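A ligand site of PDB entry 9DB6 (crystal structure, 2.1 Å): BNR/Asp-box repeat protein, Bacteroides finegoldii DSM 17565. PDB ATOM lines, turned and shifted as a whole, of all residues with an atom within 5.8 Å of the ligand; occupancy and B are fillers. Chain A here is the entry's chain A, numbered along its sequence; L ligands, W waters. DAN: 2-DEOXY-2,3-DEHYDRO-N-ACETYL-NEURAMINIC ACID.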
ATOM      1  N   ARG A 189      -9.410  -5.273  10.965  1.00  0.00           N
ATOM      2  CA  ARG A 189      -9.809  -4.039  10.309  1.00  0.00           C
ATOM      3  C   ARG A 189     -11.324  -3.882  10.333  1.00  0.00           C
ATOM      4  O   ARG A 189     -12.083  -4.848  10.495  1.00  0.00           O
ATOM      5  CB  ARG A 189      -9.312  -3.992   8.855  1.00  0.00           C
ATOM      6  CG  ARG A 189      -7.832  -3.685   8.638  1.00  0.00           C
ATOM      7  CD  ARG A 189      -7.637  -2.911   7.339  1.00  0.00           C
ATOM      8  NE  ARG A 189      -8.261  -1.593   7.412  1.00  0.00           N
ATOM      9  CZ  ARG A 189      -8.598  -0.848   6.362  1.00  0.00           C
ATOM     10  NH1 ARG A 189      -8.377  -1.244   5.128  1.00  0.00           N
ATOM     11  NH2 ARG A 189      -9.166   0.334   6.565  1.00  0.00           N
ATOM     12  N   ILE A 190     -11.767  -2.643  10.091  1.00  0.00           N
ATOM     13  CA  ILE A 190     -13.153  -2.275   9.811  1.00  0.00           C
ATOM     14  C   ILE A 190     -13.992  -2.382  11.072  1.00  0.00           C
ATOM     15  O   ILE A 190     -14.765  -3.330  11.236  1.00  0.00           O
ATOM     16  CB  ILE A 190     -13.758  -3.124   8.683  1.00  0.00           C
ATOM     17  CG1 ILE A 190     -12.742  -3.403   7.558  1.00  0.00           C
ATOM     18  CG2 ILE A 190     -14.969  -2.436   8.105  1.00  0.00           C
ATOM     19  CD1 ILE A 190     -12.158  -2.152   6.947  1.00  0.00           C
ATOM     20  N   ASP A 206     -13.385  -7.081  10.883  1.00  0.00           N
ATOM     21  CA  ASP A 206     -12.733  -8.111  10.074  1.00  0.00           C
ATOM     22  C   ASP A 206     -11.619  -8.758  10.880  1.00  0.00           C
ATOM     23  O   ASP A 206     -10.796  -8.062  11.488  1.00  0.00           O
ATOM     24  CB  ASP A 206     -12.111  -7.523   8.810  1.00  0.00           C
ATOM     25  CG  ASP A 206     -13.107  -7.225   7.710  1.00  0.00           C
ATOM     26  OD1 ASP A 206     -14.336  -7.094   7.939  1.00  0.00           O
ATOM     27  OD2 ASP A 206     -12.626  -7.095   6.572  1.00  0.00           O
ATOM     28  N   ARG A 208      -8.537 -10.585   9.655  1.00  0.00           N
ATOM     29  CA  ARG A 208      -7.816 -10.807   8.396  1.00  0.00           C
ATOM     30  C   ARG A 208      -6.553 -11.629   8.704  1.00  0.00           C
ATOM     31  O   ARG A 208      -5.487 -11.070   8.984  1.00  0.00           O
ATOM     32  CB  ARG A 208      -7.506  -9.474   7.727  1.00  0.00           C
ATOM     33  CG  ARG A 208      -8.733  -8.611   7.454  1.00  0.00           C
ATOM     34  CD  ARG A 208      -8.462  -7.435   6.527  1.00  0.00           C
ATOM     35  NE  ARG A 208      -9.697  -6.753   6.143  1.00  0.00           N
ATOM     36  CZ  ARG A 208      -9.788  -5.751   5.290  1.00  0.00           C
ATOM     37  NH1 ARG A 208      -8.712  -5.237   4.707  1.00  0.00           N
ATOM     38  NH2 ARG A 208     -10.981  -5.253   4.994  1.00  0.00           N
ATOM     39  N   ASP A 214      -7.805  -6.541   1.557  1.00  0.00           N
ATOM     40  CA  ASP A 214      -9.260  -6.669   1.537  1.00  0.00           C
ATOM     41  C   ASP A 214      -9.687  -8.020   0.942  1.00  0.00           C
ATOM     42  O   ASP A 214      -8.895  -8.746   0.342  1.00  0.00           O
ATOM     43  CB  ASP A 214      -9.899  -5.552   0.705  1.00  0.00           C
ATOM     44  CG  ASP A 214      -9.623  -4.149   1.250  1.00  0.00           C
ATOM     45  OD1 ASP A 214      -9.461  -3.964   2.473  1.00  0.00           O
ATOM     46  OD2 ASP A 214      -9.595  -3.199   0.428  1.00  0.00           O
ATOM     47  N   LEU A 215     -10.985  -8.330   1.090  1.00  0.00           N
ATOM     48  CA  LEU A 215     -11.574  -9.463   0.376  1.00  0.00           C
ATOM     49  C   LEU A 215     -11.233  -9.364  -1.114  1.00  0.00           C
ATOM     50  O   LEU A 215     -11.209  -8.269  -1.679  1.00  0.00           O
ATOM     51  CB  LEU A 215     -13.105  -9.464   0.565  1.00  0.00           C
ATOM     52  CG  LEU A 215     -13.695  -9.563   1.986  1.00  0.00           C
ATOM     53  CD1 LEU A 215     -15.192  -9.332   1.986  1.00  0.00           C
ATOM     54  CD2 LEU A 215     -13.380 -10.931   2.578  1.00  0.00           C
ATOM     55  N   ASP A 257     -16.362  -6.462   6.247  1.00  0.00           N
ATOM     56  CA  ASP A 257     -16.947  -5.117   6.258  1.00  0.00           C
ATOM     57  C   ASP A 257     -18.204  -5.092   7.128  1.00  0.00           C
ATOM     58  O   ASP A 257     -19.242  -4.592   6.686  1.00  0.00           O
ATOM     59  CB  ASP A 257     -17.250  -4.642   4.836  1.00  0.00           C
ATOM     60  CG  ASP A 257     -15.983  -4.109   4.113  1.00  0.00           C
ATOM     61  OD1 ASP A 257     -14.882  -4.267   4.644  1.00  0.00           O
ATOM     62  OD2 ASP A 257     -16.091  -3.512   3.024  1.00  0.00           O
ATOM     63  N   ALA A 284     -12.383  -8.282  -4.170  1.00  0.00           N
ATOM     64  CA  ALA A 284     -13.803  -8.405  -4.449  1.00  0.00           C
ATOM     65  C   ALA A 284     -14.332  -7.165  -5.153  1.00  0.00           C
ATOM     66  O   ALA A 284     -15.328  -7.244  -5.888  1.00  0.00           O
ATOM     67  CB  ALA A 284     -14.581  -8.644  -3.153  1.00  0.00           C
ATOM     68  N   TRP A 285     -13.705  -6.014  -4.924  1.00  0.00           N
ATOM     69  CA  TRP A 285     -14.153  -4.791  -5.567  1.00  0.00           C
ATOM     70  C   TRP A 285     -14.213  -4.943  -7.078  1.00  0.00           C
ATOM     71  O   TRP A 285     -15.061  -4.312  -7.718  1.00  0.00           O
ATOM     72  CB  TRP A 285     -13.241  -3.622  -5.188  1.00  0.00           C
ATOM     73  CG  TRP A 285     -13.844  -2.315  -5.529  1.00  0.00           C
ATOM     74  CD1 TRP A 285     -13.469  -1.482  -6.537  1.00  0.00           C
ATOM     75  CD2 TRP A 285     -14.957  -1.689  -4.872  1.00  0.00           C
ATOM     76  NE1 TRP A 285     -14.283  -0.373  -6.552  1.00  0.00           N
ATOM     77  CE2 TRP A 285     -15.200  -0.468  -5.538  1.00  0.00           C
ATOM     78  CE3 TRP A 285     -15.764  -2.037  -3.780  1.00  0.00           C
ATOM     79  CZ2 TRP A 285     -16.208   0.404  -5.157  1.00  0.00           C
ATOM     80  CZ3 TRP A 285     -16.765  -1.171  -3.404  1.00  0.00           C
ATOM     81  CH2 TRP A 285     -16.991   0.038  -4.094  1.00  0.00           C
ATOM     82  N   PHE A 329     -21.903  -5.601  -7.356  1.00  0.00           N
ATOM     83  CA  PHE A 329     -21.542  -5.748  -5.952  1.00  0.00           C
ATOM     84  C   PHE A 329     -22.623  -5.038  -5.157  1.00  0.00           C
ATOM     85  O   PHE A 329     -22.935  -3.876  -5.424  1.00  0.00           O
ATOM     86  CB  PHE A 329     -20.159  -5.105  -5.678  1.00  0.00           C
ATOM     87  CG  PHE A 329     -19.407  -5.664  -4.473  1.00  0.00           C
ATOM     88  CD1 PHE A 329     -20.031  -6.338  -3.426  1.00  0.00           C
ATOM     89  CD2 PHE A 329     -18.047  -5.459  -4.384  1.00  0.00           C
ATOM     90  CE1 PHE A 329     -19.269  -6.820  -2.340  1.00  0.00           C
ATOM     91  CE2 PHE A 329     -17.298  -5.924  -3.334  1.00  0.00           C
ATOM     92  CZ  PHE A 329     -17.906  -6.610  -2.310  1.00  0.00           C
ATOM     93  N   LEU A 331     -23.205  -4.420  -0.902  1.00  0.00           N
ATOM     94  CA  LEU A 331     -22.835  -4.706   0.478  1.00  0.00           C
ATOM     95  C   LEU A 331     -23.303  -3.594   1.399  1.00  0.00           C
ATOM     96  O   LEU A 331     -23.718  -2.522   0.952  1.00  0.00           O
ATOM     97  CB  LEU A 331     -21.315  -4.911   0.615  1.00  0.00           C
ATOM     98  CG  LEU A 331     -20.382  -3.709   0.489  1.00  0.00           C
ATOM     99  CD1 LEU A 331     -19.068  -4.019   1.186  1.00  0.00           C
ATOM    100  CD2 LEU A 331     -20.133  -3.331  -0.968  1.00  0.00           C
ATOM    101  N   GLN A 350     -24.340   0.082   0.032  1.00  0.00           N
ATOM    102  CA  GLN A 350     -23.612   0.597  -1.116  1.00  0.00           C
ATOM    103  C   GLN A 350     -23.611  -0.476  -2.201  1.00  0.00           C
ATOM    104  O   GLN A 350     -23.451  -1.659  -1.899  1.00  0.00           O
ATOM    105  CB  GLN A 350     -22.179   0.982  -0.733  1.00  0.00           C
ATOM    106  CG  GLN A 350     -21.461  -0.131   0.015  1.00  0.00           C
ATOM    107  CD  GLN A 350     -20.006   0.194   0.316  1.00  0.00           C
ATOM    108  OE1 GLN A 350     -19.341   0.945  -0.417  1.00  0.00           O
ATOM    109  NE2 GLN A 350     -19.489  -0.395   1.405  1.00  0.00           N
ATOM    110  N   THR A 383     -19.559   5.607  -1.599  1.00  0.00           N
ATOM    111  CA  THR A 383     -19.348   4.236  -1.152  1.00  0.00           C
ATOM    112  C   THR A 383     -19.826   4.062   0.298  1.00  0.00           C
ATOM    113  O   THR A 383     -21.022   3.921   0.532  1.00  0.00           O
ATOM    114  CB  THR A 383     -17.879   3.834  -1.300  1.00  0.00           C
ATOM    115  OG1 THR A 383     -17.023   4.795  -0.686  1.00  0.00           O
ATOM    116  CG2 THR A 383     -17.517   3.708  -2.776  1.00  0.00           C
ATOM    117  N   GLU A 384     -18.900   4.096   1.257  1.00  0.00           N
ATOM    118  CA  GLU A 384     -19.247   3.809   2.645  1.00  0.00           C
ATOM    119  C   GLU A 384     -19.992   4.974   3.280  1.00  0.00           C
ATOM    120  O   GLU A 384     -19.629   6.134   3.095  1.00  0.00           O
ATOM    121  CB  GLU A 384     -17.973   3.507   3.440  1.00  0.00           C
ATOM    122  CG  GLU A 384     -17.187   2.303   2.881  1.00  0.00           C
ATOM    123  CD  GLU A 384     -15.773   2.242   3.426  1.00  0.00           C
ATOM    124  OE1 GLU A 384     -15.228   3.288   3.855  1.00  0.00           O
ATOM    125  OE2 GLU A 384     -15.195   1.134   3.407  1.00  0.00           O
ATOM    126  N   ARG A 400     -18.934   8.752   2.239  1.00  0.00           N
ATOM    127  CA  ARG A 400     -17.642   8.795   1.568  1.00  0.00           C
ATOM    128  C   ARG A 400     -17.845   9.083   0.076  1.00  0.00           C
ATOM    129  O   ARG A 400     -18.500   8.314  -0.635  1.00  0.00           O
ATOM    130  CB  ARG A 400     -16.939   7.461   1.789  1.00  0.00           C
ATOM    131  CG  ARG A 400     -15.615   7.224   1.033  1.00  0.00           C
ATOM    132  CD  ARG A 400     -14.944   5.979   1.601  1.00  0.00           C
ATOM    133  NE  ARG A 400     -13.838   5.477   0.809  1.00  0.00           N
ATOM    134  CZ  ARG A 400     -12.919   4.621   1.247  1.00  0.00           C
ATOM    135  NH1 ARG A 400     -12.958   4.137   2.475  1.00  0.00           N
ATOM    136  NH2 ARG A 400     -11.955   4.223   0.415  1.00  0.00           N
ATOM    137  N   ASN A 402     -16.334   9.844  -3.670  1.00  0.00           N
ATOM    138  CA  ASN A 402     -15.143   9.642  -4.492  1.00  0.00           C
ATOM    139  C   ASN A 402     -14.711  10.902  -5.242  1.00  0.00           C
ATOM    140  O   ASN A 402     -13.639  10.896  -5.849  1.00  0.00           O
ATOM    141  CB  ASN A 402     -15.383   8.499  -5.476  1.00  0.00           C
ATOM    142  CG  ASN A 402     -15.174   7.144  -4.834  1.00  0.00           C
ATOM    143  OD1 ASN A 402     -14.455   7.030  -3.857  1.00  0.00           O
ATOM    144  ND2 ASN A 402     -15.800   6.113  -5.398  1.00  0.00           N
ATOM    145  N   ARG A 464      -4.425   9.275   6.219  1.00  0.00           N
ATOM    146  CA  ARG A 464      -5.292   8.736   7.264  1.00  0.00           C
ATOM    147  C   ARG A 464      -4.568   8.884   8.590  1.00  0.00           C
ATOM    148  O   ARG A 464      -3.919   7.962   9.088  1.00  0.00           O
ATOM    149  CB  ARG A 464      -5.678   7.299   6.958  1.00  0.00           C
ATOM    150  CG  ARG A 464      -6.495   7.204   5.671  1.00  0.00           C
ATOM    151  CD  ARG A 464      -7.074   5.807   5.534  1.00  0.00           C
ATOM    152  NE  ARG A 464      -7.838   5.645   4.314  1.00  0.00           N
ATOM    153  CZ  ARG A 464      -8.338   4.495   3.905  1.00  0.00           C
ATOM    154  NH1 ARG A 464      -8.230   3.398   4.654  1.00  0.00           N
ATOM    155  NH2 ARG A 464      -8.957   4.430   2.729  1.00  0.00           N
ATOM    156  N   TRP A 493      -4.948   3.204   9.738  1.00  0.00           N
ATOM    157  CA  TRP A 493      -5.798   2.778   8.622  1.00  0.00           C
ATOM    158  C   TRP A 493      -7.134   3.532   8.560  1.00  0.00           C
ATOM    159  O   TRP A 493      -7.834   3.449   7.543  1.00  0.00           O
ATOM    160  CB  TRP A 493      -6.006   1.263   8.685  1.00  0.00           C
ATOM    161  CG  TRP A 493      -4.748   0.492   8.296  1.00  0.00           C
ATOM    162  CD1 TRP A 493      -3.711   0.951   7.535  1.00  0.00           C
ATOM    163  CD2 TRP A 493      -4.395  -0.852   8.689  1.00  0.00           C
ATOM    164  NE1 TRP A 493      -2.739  -0.030   7.415  1.00  0.00           N
ATOM    165  CE2 TRP A 493      -3.134  -1.142   8.114  1.00  0.00           C
ATOM    166  CE3 TRP A 493      -5.004  -1.839   9.472  1.00  0.00           C
ATOM    167  CZ2 TRP A 493      -2.497  -2.379   8.278  1.00  0.00           C
ATOM    168  CZ3 TRP A 493      -4.382  -3.052   9.629  1.00  0.00           C
ATOM    169  CH2 TRP A 493      -3.138  -3.314   9.040  1.00  0.00           C
ATOM    170  N   TYR A 495     -10.334   3.919   9.872  1.00  0.00           N
ATOM    171  CA  TYR A 495     -11.746   3.665  10.150  1.00  0.00           C
ATOM    172  C   TYR A 495     -12.048   3.809  11.641  1.00  0.00           C
ATOM    173  O   TYR A 495     -11.193   3.569  12.498  1.00  0.00           O
ATOM    174  CB  TYR A 495     -12.147   2.265   9.664  1.00  0.00           C
ATOM    175  CG  TYR A 495     -12.284   2.119   8.170  1.00  0.00           C
ATOM    176  CD1 TYR A 495     -11.421   2.772   7.302  1.00  0.00           C
ATOM    177  CD2 TYR A 495     -13.271   1.304   7.617  1.00  0.00           C
ATOM    178  CE1 TYR A 495     -11.550   2.629   5.931  1.00  0.00           C
ATOM    179  CE2 TYR A 495     -13.397   1.145   6.271  1.00  0.00           C
ATOM    180  CZ  TYR A 495     -12.537   1.810   5.424  1.00  0.00           C
ATOM    181  OH  TYR A 495     -12.643   1.650   4.062  1.00  0.00           O
HETATM  182  C1  DAN L   1     -10.286   0.942   2.546  1.00  0.00           C
HETATM  183  C2  DAN L   1     -11.423  -0.032   2.056  1.00  0.00           C
HETATM  184  C3  DAN L   1     -11.921  -1.147   2.574  1.00  0.00           C
HETATM  185  C4  DAN L   1     -12.899  -2.098   1.878  1.00  0.00           C
HETATM  186  C6  DAN L   1     -13.020  -0.418   0.429  1.00  0.00           C
HETATM  187  C9  DAN L   1     -13.997   2.054  -2.427  1.00  0.00           C
HETATM  188  C10 DAN L   1     -13.973  -3.995  -0.193  1.00  0.00           C
HETATM  189  C11 DAN L   1     -15.041  -4.686  -0.929  1.00  0.00           C
HETATM  190  O1A DAN L   1      -9.971   1.767   1.689  1.00  0.00           O
HETATM  191  O1B DAN L   1      -9.757   0.856   3.671  1.00  0.00           O
HETATM  192  O4  DAN L   1     -12.707  -3.366   2.496  1.00  0.00           O
HETATM  193  O6  DAN L   1     -11.876   0.317   0.854  1.00  0.00           O
HETATM  194  O8  DAN L   1     -14.426   2.197  -0.086  1.00  0.00           O
HETATM  195  O9  DAN L   1     -13.038   1.901  -3.434  1.00  0.00           O
HETATM  196  O10 DAN L   1     -13.243  -4.553   0.590  1.00  0.00           O
HETATM  197  O   HOH W   1     -14.488   5.076  -1.862  1.00  0.00           O
HETATM  198  O   HOH W   2     -16.673   0.182  -0.286  1.00  0.00           O
HETATM  199  O   HOH W   3     -12.087  -5.743  -2.329  1.00  0.00           O
HETATM  200  O   HOH W   4     -14.746   3.534  -5.180  1.00  0.00           O
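Water W4 lies within hydrogen-bond range of the side-chain amide nitrogen of Asn 402 (2.8 Å) and an oxygen (O9) of the ligand (2.9 Å). Water W2 lies within hydrogen-bond range of the side-chain amide oxygen (OE1) of Gln 350 and an oxygen (O8) of the ligand. Water W1 lies within hydrogen-bond range of NE of Arg 400 (2.8 Å), OD1 of Asn 402 (2.8 Å), OG1 of Thr 383 (2.8 Å) and O8 of the ligand (3.4 Å). Water W3 lies within hydrogen-bond range of the backbone carbonyl oxygen of Leu 215 (2.8 Å), the backbone NH of Trp 285 (3.1 Å), the backbone NH of Ala 284 (3.2 Å) and an oxygen (O10) of the ligand (3.4 Å).
OH of Tyr 495 lies close to O1B of the ligand, 3.0 Å away. The guanidinium group of Arg 189 lies within salt-bridge range of an oxygen (O1B) of the ligand (2.9 Å). An oxygen (O1A) of the ligand is in salt-bridge range of the guanidinium group of Arg 464 (3.0 Å). The guanidinium group (NH2) of Arg 400 is in salt-bridge range of an oxygen (O1A) of the ligand, at 3.4 Å. The side-chain carboxylate (OD1) of Asp 257 lies within hydrogen-bond range of an oxygen (O4) of the ligand, at 3.2 Å. An oxygen (O4) of the ligand sits at hydrogen-bond distance from the side-chain carboxylate (OD1) of Asp 214 (3.3 Å).
The side-chain hydroxyl (OH) of Tyr 495 is in hydrogen-bond range of the side-chain carboxylate (OE2) of Glu 384 (2.7 Å). OD1 of Asp 214 lies within salt-bridge range of NH1 of Arg 189 (3.95 Å). O of Arg 189 sits at hydrogen-bond distance from N of Asp 206. The guanidinium group of Arg 464 lies within hydrogen-bond range of the backbone carbonyl oxygen of Trp 493. The backbone NH of Thr 383 lies within hydrogen-bond range of the backbone carbonyl oxygen of Arg 400, at 3.1 Å. OD1 of Asp 206 is in hydrogen-bond range of N of Asp 257 (2.7 Å). OD1 of Asp 214 is in salt-bridge range of NH1 of Arg 208, at 2.7 Å. OD2 of Asp 206 is in salt-bridge range of NH2 of Arg 208.
Residues that only touch the ligand: Phe 329, Arg 208, Thr 383, Glu 384 and Trp 285. Hydrophobic or aromatic side chains that line the ligand: Trp 285, Phe 329 and Tyr 495. Within 4 Å of the ligand: Arg 189, Arg 208, Asp 214, Asp 257, Trp 285, Phe 329, Thr 383, Glu 384, Arg 400, Arg 464 and Tyr 495.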
